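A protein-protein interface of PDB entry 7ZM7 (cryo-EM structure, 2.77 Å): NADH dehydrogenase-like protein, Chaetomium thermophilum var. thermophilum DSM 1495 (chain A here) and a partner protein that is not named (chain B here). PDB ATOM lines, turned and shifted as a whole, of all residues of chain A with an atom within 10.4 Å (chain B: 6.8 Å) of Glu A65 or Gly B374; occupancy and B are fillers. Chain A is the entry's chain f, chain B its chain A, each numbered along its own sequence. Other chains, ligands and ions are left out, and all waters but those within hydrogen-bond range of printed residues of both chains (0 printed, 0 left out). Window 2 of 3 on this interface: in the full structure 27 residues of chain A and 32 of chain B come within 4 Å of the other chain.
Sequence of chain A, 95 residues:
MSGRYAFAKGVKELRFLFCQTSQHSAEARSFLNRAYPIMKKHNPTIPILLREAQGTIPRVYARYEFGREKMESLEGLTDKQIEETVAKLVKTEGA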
ATOM      1  N   ALA A   8       2.248 -39.464 -12.650  1.00  0.00           N
ATOM      2  CA  ALA A   8       1.851 -39.728 -14.023  1.00  0.00           C
ATOM      3  C   ALA A   8       2.059 -38.486 -14.873  1.00  0.00           C
ATOM      4  O   ALA A   8       1.735 -37.371 -14.458  1.00  0.00           O
ATOM      5  CB  ALA A   8       0.390 -40.169 -14.079  1.00  0.00           C
ATOM      6  N   LYS A   9       2.615 -38.685 -16.068  1.00  0.00           N
ATOM      7  CA  LYS A   9       2.811 -37.573 -16.984  1.00  0.00           C
ATOM      8  C   LYS A   9       1.478 -36.903 -17.265  1.00  0.00           C
ATOM      9  O   LYS A   9       0.464 -37.572 -17.482  1.00  0.00           O
ATOM     10  CB  LYS A   9       3.443 -38.054 -18.286  1.00  0.00           C
ATOM     11  CG  LYS A   9       3.687 -36.942 -19.291  1.00  0.00           C
ATOM     12  CD  LYS A   9       4.404 -37.462 -20.522  1.00  0.00           C
ATOM     13  CE  LYS A   9       3.461 -38.259 -21.409  1.00  0.00           C
ATOM     14  NZ  LYS A   9       2.458 -37.385 -22.076  1.00  0.00           N
ATOM     15  N   GLY A  10       1.477 -35.578 -17.246  1.00  0.00           N
ATOM     16  CA  GLY A  10       0.250 -34.813 -17.293  1.00  0.00           C
ATOM     17  C   GLY A  10      -0.114 -34.162 -15.982  1.00  0.00           C
ATOM     18  O   GLY A  10      -1.144 -33.486 -15.910  1.00  0.00           O
ATOM     19  N   VAL A  11       0.661 -34.359 -14.944  1.00  0.00           N
ATOM     20  CA  VAL A  11       0.492 -33.628 -13.699  1.00  0.00           C
ATOM     21  C   VAL A  11       1.505 -32.495 -13.669  1.00  0.00           C
ATOM     22  O   VAL A  11       2.674 -32.665 -14.030  1.00  0.00           O
ATOM     23  CB  VAL A  11       0.633 -34.561 -12.485  1.00  0.00           C
ATOM     24  CG1 VAL A  11       2.070 -34.936 -12.280  1.00  0.00           C
ATOM     25  CG2 VAL A  11       0.060 -33.904 -11.243  1.00  0.00           C
ATOM     26  N   LYS A  12       1.048 -31.319 -13.260  1.00  0.00           N
ATOM     27  CA  LYS A  12       1.858 -30.120 -13.385  1.00  0.00           C
ATOM     28  C   LYS A  12       2.365 -29.558 -12.071  1.00  0.00           C
ATOM     29  O   LYS A  12       3.446 -28.981 -12.055  1.00  0.00           O
ATOM     30  CB  LYS A  12       1.071 -29.037 -14.127  1.00  0.00           C
ATOM     31  CG  LYS A  12       0.706 -29.458 -15.520  1.00  0.00           C
ATOM     32  CD  LYS A  12       1.940 -29.558 -16.385  1.00  0.00           C
ATOM     33  CE  LYS A  12       1.599 -29.988 -17.790  1.00  0.00           C
ATOM     34  NZ  LYS A  12       0.836 -28.939 -18.510  1.00  0.00           N
ATOM     35  N   GLU A  13       1.632 -29.708 -10.975  1.00  0.00           N
ATOM     36  CA  GLU A  13       2.035 -29.068  -9.732  1.00  0.00           C
ATOM     37  C   GLU A  13       1.177 -29.590  -8.599  1.00  0.00           C
ATOM     38  O   GLU A  13      -0.046 -29.658  -8.732  1.00  0.00           O
ATOM     39  CB  GLU A  13       1.908 -27.541  -9.854  1.00  0.00           C
ATOM     40  CG  GLU A  13       1.886 -26.769  -8.554  1.00  0.00           C
ATOM     41  CD  GLU A  13       1.720 -25.283  -8.803  1.00  0.00           C
ATOM     42  OE1 GLU A  13       1.353 -24.545  -7.866  1.00  0.00           O
ATOM     43  OE2 GLU A  13       1.950 -24.850  -9.951  1.00  0.00           O
ATOM     44  N   ALA A  62      -3.813 -30.909  -7.014  1.00  0.00           N
ATOM     45  CA  ALA A  62      -3.041 -31.482  -8.107  1.00  0.00           C
ATOM     46  C   ALA A  62      -3.466 -30.791  -9.387  1.00  0.00           C
ATOM     47  O   ALA A  62      -4.653 -30.765  -9.714  1.00  0.00           O
ATOM     48  CB  ALA A  62      -3.233 -32.993  -8.209  1.00  0.00           C
ATOM     49  N   ARG A  63      -2.506 -30.218 -10.090  1.00  0.00           N
ATOM     50  CA  ARG A  63      -2.791 -29.504 -11.316  1.00  0.00           C
ATOM     51  C   ARG A  63      -2.273 -30.301 -12.498  1.00  0.00           C
ATOM     52  O   ARG A  63      -1.274 -31.015 -12.418  1.00  0.00           O
ATOM     53  CB  ARG A  63      -2.172 -28.106 -11.308  1.00  0.00           C
ATOM     54  CG  ARG A  63      -3.000 -27.074 -12.040  1.00  0.00           C
ATOM     55  CD  ARG A  63      -2.327 -25.705 -12.101  1.00  0.00           C
ATOM     56  NE  ARG A  63      -1.253 -25.655 -13.083  1.00  0.00           N
ATOM     57  CZ  ARG A  63       0.005 -25.348 -12.802  1.00  0.00           C
ATOM     58  NH1 ARG A  63       0.916 -25.329 -13.758  1.00  0.00           N
ATOM     59  NH2 ARG A  63       0.349 -25.052 -11.561  1.00  0.00           N
ATOM     60  N   TYR A  64      -2.993 -30.181 -13.601  1.00  0.00           N
ATOM     61  CA  TYR A  64      -2.680 -30.896 -14.818  1.00  0.00           C
ATOM     62  C   TYR A  64      -2.650 -29.878 -15.945  1.00  0.00           C
ATOM     63  O   TYR A  64      -2.682 -28.667 -15.713  1.00  0.00           O
ATOM     64  CB  TYR A  64      -3.691 -32.025 -15.034  1.00  0.00           C
ATOM     65  CG  TYR A  64      -4.080 -32.725 -13.762  1.00  0.00           C
ATOM     66  CD1 TYR A  64      -3.290 -33.726 -13.232  1.00  0.00           C
ATOM     67  CD2 TYR A  64      -5.223 -32.370 -13.081  1.00  0.00           C
ATOM     68  CE1 TYR A  64      -3.634 -34.366 -12.074  1.00  0.00           C
ATOM     69  CE2 TYR A  64      -5.571 -32.998 -11.922  1.00  0.00           C
ATOM     70  CZ  TYR A  64      -4.772 -33.995 -11.419  1.00  0.00           C
ATOM     71  OH  TYR A  64      -5.124 -34.628 -10.256  1.00  0.00           O
ATOM     72  N   GLU A  65      -2.589 -30.368 -17.172  1.00  0.00           N
ATOM     73  CA  GLU A  65      -2.451 -29.498 -18.326  1.00  0.00           C
ATOM     74  C   GLU A  65      -3.782 -28.768 -18.551  1.00  0.00           C
ATOM     75  O   GLU A  65      -4.830 -29.196 -18.059  1.00  0.00           O
ATOM     76  CB  GLU A  65      -2.028 -30.370 -19.506  1.00  0.00           C
ATOM     77  CG  GLU A  65      -1.559 -29.727 -20.786  1.00  0.00           C
ATOM     78  CD  GLU A  65      -2.632 -29.299 -21.734  1.00  0.00           C
ATOM     79  OE1 GLU A  65      -3.732 -29.888 -21.756  1.00  0.00           O
ATOM     80  OE2 GLU A  65      -2.298 -28.420 -22.547  1.00  0.00           O
ATOM     81  N   PHE A  66      -3.734 -27.623 -19.245  1.00  0.00           N
ATOM     82  CA  PHE A  66      -4.885 -26.714 -19.387  1.00  0.00           C
ATOM     83  C   PHE A  66      -5.417 -26.188 -18.064  1.00  0.00           C
ATOM     84  O   PHE A  66      -6.549 -25.709 -18.005  1.00  0.00           O
ATOM     85  CB  PHE A  66      -6.043 -27.339 -20.178  1.00  0.00           C
ATOM     86  CG  PHE A  66      -5.773 -27.526 -21.635  1.00  0.00           C
ATOM     87  CD1 PHE A  66      -4.721 -26.877 -22.252  1.00  0.00           C
ATOM     88  CD2 PHE A  66      -6.573 -28.365 -22.391  1.00  0.00           C
ATOM     89  CE1 PHE A  66      -4.493 -27.040 -23.611  1.00  0.00           C
ATOM     90  CE2 PHE A  66      -6.339 -28.546 -23.739  1.00  0.00           C
ATOM     91  CZ  PHE A  66      -5.293 -27.887 -24.349  1.00  0.00           C
ATOM     92  N   GLY A  67      -4.628 -26.236 -17.001  1.00  0.00           N
ATOM     93  CA  GLY A  67      -5.059 -25.663 -15.744  1.00  0.00           C
ATOM     94  C   GLY A  67      -6.237 -26.335 -15.084  1.00  0.00           C
ATOM     95  O   GLY A  67      -7.039 -25.655 -14.443  1.00  0.00           O
ATOM     96  N   ARG A  68      -6.374 -27.647 -15.221  1.00  0.00           N
ATOM     97  CA  ARG A  68      -7.407 -28.380 -14.504  1.00  0.00           C
ATOM     98  C   ARG A  68      -6.853 -28.818 -13.164  1.00  0.00           C
ATOM     99  O   ARG A  68      -5.723 -29.302 -13.079  1.00  0.00           O
ATOM    100  CB  ARG A  68      -7.876 -29.584 -15.308  1.00  0.00           C
ATOM    101  CG  ARG A  68      -8.924 -30.429 -14.612  1.00  0.00           C
ATOM    102  CD  ARG A  68      -9.415 -31.534 -15.521  1.00  0.00           C
ATOM    103  NE  ARG A  68      -8.316 -32.394 -15.940  1.00  0.00           N
ATOM    104  CZ  ARG A  68      -7.935 -33.490 -15.297  1.00  0.00           C
ATOM    105  NH1 ARG A  68      -6.913 -34.205 -15.751  1.00  0.00           N
ATOM    106  NH2 ARG A  68      -8.572 -33.872 -14.201  1.00  0.00           N
ATOM    107  N   GLU A  69      -7.628 -28.623 -12.113  1.00  0.00           N
ATOM    108  CA  GLU A  69      -7.110 -28.760 -10.768  1.00  0.00           C
ATOM    109  C   GLU A  69      -8.104 -29.521  -9.905  1.00  0.00           C
ATOM    110  O   GLU A  69      -9.311 -29.280  -9.959  1.00  0.00           O
ATOM    111  CB  GLU A  69      -6.814 -27.374 -10.195  1.00  0.00           C
ATOM    112  CG  GLU A  69      -6.138 -27.326  -8.841  1.00  0.00           C
ATOM    113  CD  GLU A  69      -5.771 -25.904  -8.461  1.00  0.00           C
ATOM    114  OE1 GLU A  69      -6.074 -24.983  -9.245  1.00  0.00           O
ATOM    115  OE2 GLU A  69      -5.168 -25.702  -7.392  1.00  0.00           O
ATOM    116  N   LYS A  70      -7.587 -30.443  -9.107  1.00  0.00           N
ATOM    117  CA  LYS A  70      -8.399 -31.261  -8.225  1.00  0.00           C
ATOM    118  C   LYS A  70      -7.969 -31.047  -6.786  1.00  0.00           C
ATOM    119  O   LYS A  70      -6.778 -30.971  -6.489  1.00  0.00           O
ATOM    120  CB  LYS A  70      -8.284 -32.741  -8.583  1.00  0.00           C
ATOM    121  CG  LYS A  70      -9.117 -33.628  -7.687  1.00  0.00           C
ATOM    122  CD  LYS A  70     -10.595 -33.387  -7.910  1.00  0.00           C
ATOM    123  CE  LYS A  70     -11.429 -34.379  -7.127  1.00  0.00           C
ATOM    124  NZ  LYS A  70     -11.264 -34.154  -5.662  1.00  0.00           N
ATOM    125  N   LEU A  89      -4.387 -38.923  -6.883  1.00  0.00           N
ATOM    126  CA  LEU A  89      -4.235 -37.656  -7.579  1.00  0.00           C
ATOM    127  C   LEU A  89      -3.091 -37.660  -8.573  1.00  0.00           C
ATOM    128  O   LEU A  89      -3.061 -36.815  -9.465  1.00  0.00           O
ATOM    129  CB  LEU A  89      -4.015 -36.531  -6.568  1.00  0.00           C
ATOM    130  CG  LEU A  89      -5.234 -35.838  -5.969  1.00  0.00           C
ATOM    131  CD1 LEU A  89      -5.919 -35.005  -7.012  1.00  0.00           C
ATOM    132  CD2 LEU A  89      -6.211 -36.831  -5.382  1.00  0.00           C
ATOM    133  N   TYR B 340      -2.717 -14.041 -31.702  1.00  0.00           N
ATOM    134  CA  TYR B 340      -2.562 -15.311 -31.010  1.00  0.00           C
ATOM    135  C   TYR B 340      -3.155 -16.454 -31.815  1.00  0.00           C
ATOM    136  O   TYR B 340      -2.587 -17.548 -31.860  1.00  0.00           O
ATOM    137  CB  TYR B 340      -3.205 -15.243 -29.626  1.00  0.00           C
ATOM    138  CG  TYR B 340      -2.865 -16.433 -28.776  1.00  0.00           C
ATOM    139  CD1 TYR B 340      -1.629 -16.542 -28.164  1.00  0.00           C
ATOM    140  CD2 TYR B 340      -3.771 -17.462 -28.606  1.00  0.00           C
ATOM    141  CE1 TYR B 340      -1.318 -17.633 -27.387  1.00  0.00           C
ATOM    142  CE2 TYR B 340      -3.464 -18.560 -27.833  1.00  0.00           C
ATOM    143  CZ  TYR B 340      -2.237 -18.640 -27.232  1.00  0.00           C
ATOM    144  OH  TYR B 340      -1.933 -19.735 -26.466  1.00  0.00           O
ATOM    145  N   LYS B 346       2.086 -23.644 -29.508  1.00  0.00           N
ATOM    146  CA  LYS B 346       2.060 -24.975 -28.928  1.00  0.00           C
ATOM    147  C   LYS B 346       2.278 -24.872 -27.421  1.00  0.00           C
ATOM    148  O   LYS B 346       2.230 -23.787 -26.837  1.00  0.00           O
ATOM    149  CB  LYS B 346       3.104 -25.867 -29.596  1.00  0.00           C
ATOM    150  CG  LYS B 346       2.994 -25.930 -31.110  1.00  0.00           C
ATOM    151  CD  LYS B 346       1.740 -26.664 -31.546  1.00  0.00           C
ATOM    152  CE  LYS B 346       0.729 -25.708 -32.157  1.00  0.00           C
ATOM    153  NZ  LYS B 346      -0.484 -26.408 -32.655  1.00  0.00           N
ATOM    154  N   GLU B 347       2.510 -26.010 -26.774  1.00  0.00           N
ATOM    155  CA  GLU B 347       2.725 -26.020 -25.335  1.00  0.00           C
ATOM    156  C   GLU B 347       3.979 -25.235 -24.983  1.00  0.00           C
ATOM    157  O   GLU B 347       5.054 -25.475 -25.537  1.00  0.00           O
ATOM    158  CB  GLU B 347       2.838 -27.460 -24.839  1.00  0.00           C
ATOM    159  CG  GLU B 347       2.902 -27.613 -23.332  1.00  0.00           C
ATOM    160  CD  GLU B 347       2.807 -29.063 -22.893  1.00  0.00           C
ATOM    161  OE1 GLU B 347       2.738 -29.947 -23.772  1.00  0.00           O
ATOM    162  OE2 GLU B 347       2.795 -29.319 -21.671  1.00  0.00           O
ATOM    163  N   ASN B 348       3.827 -24.287 -24.060  1.00  0.00           N
ATOM    164  CA  ASN B 348       4.877 -23.436 -23.507  1.00  0.00           C
ATOM    165  C   ASN B 348       5.431 -22.420 -24.492  1.00  0.00           C
ATOM    166  O   ASN B 348       6.445 -21.787 -24.199  1.00  0.00           O
ATOM    167  CB  ASN B 348       6.029 -24.263 -22.932  1.00  0.00           C
ATOM    168  CG  ASN B 348       5.590 -25.143 -21.797  1.00  0.00           C
ATOM    169  OD1 ASN B 348       4.680 -24.794 -21.050  1.00  0.00           O
ATOM    170  ND2 ASN B 348       6.233 -26.293 -21.654  1.00  0.00           N
ATOM    171  N   GLU B 349       4.804 -22.241 -25.647  1.00  0.00           N
ATOM    172  CA  GLU B 349       5.240 -21.222 -26.594  1.00  0.00           C
ATOM    173  C   GLU B 349       4.726 -19.830 -26.246  1.00  0.00           C
ATOM    174  O   GLU B 349       5.216 -18.852 -26.811  1.00  0.00           O
ATOM    175  CB  GLU B 349       4.793 -21.595 -28.010  1.00  0.00           C
ATOM    176  CG  GLU B 349       5.678 -22.640 -28.675  1.00  0.00           C
ATOM    177  CD  GLU B 349       5.347 -22.849 -30.144  1.00  0.00           C
ATOM    178  OE1 GLU B 349       4.146 -22.885 -30.488  1.00  0.00           O
ATOM    179  OE2 GLU B 349       6.288 -22.982 -30.954  1.00  0.00           O
ATOM    180  N   PHE B 350       3.758 -19.723 -25.345  1.00  0.00           N
ATOM    181  CA  PHE B 350       3.322 -18.450 -24.793  1.00  0.00           C
ATOM    182  C   PHE B 350       4.093 -18.194 -23.506  1.00  0.00           C
ATOM    183  O   PHE B 350       3.965 -18.951 -22.546  1.00  0.00           O
ATOM    184  CB  PHE B 350       1.815 -18.474 -24.537  1.00  0.00           C
ATOM    185  CG  PHE B 350       1.325 -17.353 -23.690  1.00  0.00           C
ATOM    186  CD1 PHE B 350       1.039 -16.124 -24.242  1.00  0.00           C
ATOM    187  CD2 PHE B 350       1.136 -17.532 -22.333  1.00  0.00           C
ATOM    188  CE1 PHE B 350       0.584 -15.094 -23.457  1.00  0.00           C
ATOM    189  CE2 PHE B 350       0.688 -16.503 -21.536  1.00  0.00           C
ATOM    190  CZ  PHE B 350       0.413 -15.284 -22.102  1.00  0.00           C
ATOM    191  N   LEU B 369      -4.253 -17.644 -16.698  1.00  0.00           N
ATOM    192  CA  LEU B 369      -4.424 -17.502 -18.139  1.00  0.00           C
ATOM    193  C   LEU B 369      -3.277 -18.145 -18.886  1.00  0.00           C
ATOM    194  O   LEU B 369      -3.457 -18.673 -19.987  1.00  0.00           O
ATOM    195  CB  LEU B 369      -4.544 -16.031 -18.520  1.00  0.00           C
ATOM    196  CG  LEU B 369      -4.687 -15.817 -20.027  1.00  0.00           C
ATOM    197  CD1 LEU B 369      -6.074 -16.215 -20.474  1.00  0.00           C
ATOM    198  CD2 LEU B 369      -4.378 -14.407 -20.428  1.00  0.00           C
ATOM    199  N   ALA B 370      -2.082 -18.099 -18.309  1.00  0.00           N
ATOM    200  CA  ALA B 370      -0.979 -18.861 -18.868  1.00  0.00           C
ATOM    201  C   ALA B 370      -1.279 -20.352 -18.849  1.00  0.00           C
ATOM    202  O   ALA B 370      -1.023 -21.051 -19.832  1.00  0.00           O
ATOM    203  CB  ALA B 370       0.301 -18.559 -18.098  1.00  0.00           C
ATOM    204  N   ASN B 371      -1.825 -20.856 -17.742  1.00  0.00           N
ATOM    205  CA  ASN B 371      -2.064 -22.289 -17.627  1.00  0.00           C
ATOM    206  C   ASN B 371      -3.130 -22.754 -18.602  1.00  0.00           C
ATOM    207  O   ASN B 371      -2.984 -23.810 -19.229  1.00  0.00           O
ATOM    208  CB  ASN B 371      -2.470 -22.658 -16.207  1.00  0.00           C
ATOM    209  CG  ASN B 371      -1.329 -22.600 -15.250  1.00  0.00           C
ATOM    210  OD1 ASN B 371      -0.172 -22.522 -15.644  1.00  0.00           O
ATOM    211  ND2 ASN B 371      -1.645 -22.632 -13.971  1.00  0.00           N
ATOM    212  N   ARG B 372      -4.205 -21.982 -18.756  1.00  0.00           N
ATOM    213  CA  ARG B 372      -5.250 -22.357 -19.697  1.00  0.00           C
ATOM    214  C   ARG B 372      -4.781 -22.308 -21.137  1.00  0.00           C
ATOM    215  O   ARG B 372      -5.519 -22.742 -22.023  1.00  0.00           O
ATOM    216  CB  ARG B 372      -6.467 -21.453 -19.546  1.00  0.00           C
ATOM    217  CG  ARG B 372      -6.699 -20.942 -18.169  1.00  0.00           C
ATOM    218  CD  ARG B 372      -7.437 -21.930 -17.326  1.00  0.00           C
ATOM    219  NE  ARG B 372      -7.930 -21.313 -16.098  1.00  0.00           N
ATOM    220  CZ  ARG B 372      -7.316 -21.386 -14.922  1.00  0.00           C
ATOM    221  NH1 ARG B 372      -7.847 -20.797 -13.863  1.00  0.00           N
ATOM    222  NH2 ARG B 372      -6.181 -22.049 -14.794  1.00  0.00           N
ATOM    223  N   LEU B 373      -3.607 -21.746 -21.398  1.00  0.00           N
ATOM    224  CA  LEU B 373      -3.032 -21.709 -22.731  1.00  0.00           C
ATOM    225  C   LEU B 373      -1.947 -22.752 -22.909  1.00  0.00           C
ATOM    226  O   LEU B 373      -1.216 -22.711 -23.898  1.00  0.00           O
ATOM    227  CB  LEU B 373      -2.479 -20.324 -23.030  1.00  0.00           C
ATOM    228  CG  LEU B 373      -3.521 -19.240 -23.252  1.00  0.00           C
ATOM    229  CD1 LEU B 373      -2.842 -17.893 -23.375  1.00  0.00           C
ATOM    230  CD2 LEU B 373      -4.380 -19.543 -24.451  1.00  0.00           C
ATOM    231  N   GLY B 374      -1.825 -23.682 -21.975  1.00  0.00           N
ATOM    232  CA  GLY B 374      -0.849 -24.732 -22.127  1.00  0.00           C
ATOM    233  C   GLY B 374       0.570 -24.305 -21.876  1.00  0.00           C
ATOM    234  O   GLY B 374       1.498 -24.999 -22.289  1.00  0.00           O
ATOM    235  N   SER B 375       0.777 -23.189 -21.194  1.00  0.00           N
ATOM    236  CA  SER B 375       2.118 -22.697 -20.936  1.00  0.00           C
ATOM    237  C   SER B 375       2.369 -22.670 -19.439  1.00  0.00           C
ATOM    238  O   SER B 375       1.514 -22.233 -18.665  1.00  0.00           O
ATOM    239  CB  SER B 375       2.319 -21.308 -21.544  1.00  0.00           C
ATOM    240  OG  SER B 375       3.583 -20.764 -21.203  1.00  0.00           O
ATOM    241  N   GLU B 376       3.525 -23.189 -19.040  1.00  0.00           N
ATOM    242  CA  GLU B 376       4.083 -22.968 -17.718  1.00  0.00           C
ATOM    243  C   GLU B 376       5.281 -22.035 -17.767  1.00  0.00           C
ATOM    244  O   GLU B 376       5.995 -21.895 -16.772  1.00  0.00           O
ATOM    245  CB  GLU B 376       4.463 -24.302 -17.081  1.00  0.00           C
ATOM    246  CG  GLU B 376       3.318 -24.985 -16.356  1.00  0.00           C
ATOM    247  CD  GLU B 376       2.187 -25.398 -17.282  1.00  0.00           C
ATOM    248  OE1 GLU B 376       2.469 -25.885 -18.396  1.00  0.00           O
ATOM    249  OE2 GLU B 376       1.014 -25.227 -16.898  1.00  0.00           O
ATOM    250  N   ASN B 377       5.509 -21.388 -18.905  1.00  0.00           N
ATOM    251  CA  ASN B 377       6.669 -20.537 -19.138  1.00  0.00           C
ATOM    252  C   ASN B 377       6.451 -19.218 -18.411  1.00  0.00           C
ATOM    253  O   ASN B 377       5.930 -18.254 -18.969  1.00  0.00           O
ATOM    254  CB  ASN B 377       6.862 -20.327 -20.631  1.00  0.00           C
ATOM    255  CG  ASN B 377       8.237 -19.862 -20.979  1.00  0.00           C
ATOM    256  OD1 ASN B 377       9.044 -19.590 -20.105  1.00  0.00           O
ATOM    257  ND2 ASN B 377       8.517 -19.764 -22.262  1.00  0.00           N
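Of the 16 printed residues of chain A, 5 touch a printed residue of chain B.
Along chain A the printed residues that touch a printed residue of chain B span positions 12 to 67.
The side-chain amide oxygen of Asn B371 sits close to the backbone carbonyl oxygen of Ser B375 (3.5 Å).
The backbone NH (N) of Asn B348 sits at hydrogen-bond distance from the backbone carbonyl oxygen (O) of Gly B374, 3.0 Å away.
The side-chain carboxylate (OE2) of Glu B376 sits close to the side-chain amide oxygen (OD1) of Asn B371, at 3.2 Å.
The backbone carbonyl oxygen (O) of Arg A63 lies within hydrogen-bond range of the backbone NH (N) of Lys A12 (2.5 Å).
OE1 of Glu A13 is in salt-bridge range of NH2 of Arg A63 (3.9 Å).
The backbone NH (N) of Glu B376 is in hydrogen-bond range of the side-chain amide oxygen (OD1) of Asn B348 (2.8 Å).
OE2 of Glu A65 touches CA of Gly B374, 3.98 Å away.
O of Asn B371 touches CA of Phe A66, 3.5 Å away.
CD of Arg B372 touches O of Phe A66, 3.9 Å away.
N of Gly A67 touches O of Asn B371, 3.7 Å away.
Gly A67 touches Arg B372.
The guanidinium group (NE) of Arg A63 lies close to the side-chain amide nitrogen (ND2) of Asn B371.
The side-chain amino group (NZ) of Lys A12 lies within salt-bridge range of the side-chain carboxylate (OE2) of Glu B347, 3.7 Å away.
NH1 of Arg A63 lies within salt-bridge range of OE2 of Glu B376 (3.1 Å).
NZ of Lys A12 is in salt-bridge range of OE1 of Glu B376, at 3.5 Å.
Of the printed residues of chain B, Glu A65 touches Gly B374 (3.98 Å).
Printed residues of chain A within 4 Å of Gly B374: Glu A65 (3.98 Å).
No residue of chain A comes within 4 Å of Asn B348.
No residue of chain A comes within 4 Å of Ser B375.
Of the printed residues of chain B, Arg A63 touches Asn B371 and Glu B376.
Printed residues of chain A within 4 Å of Asn B371: Arg A63, Phe A66 and Gly A67.
Printed residues of chain A within 4 Å of Glu B376: Lys A12 (3.5 Å) and Arg A63 (3.1 Å).
Lys A70 touches none of the printed residues of chain B.
The nearest printed residue of chain A that does not touch Arg B372 is Arg A68 (5.6 Å).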
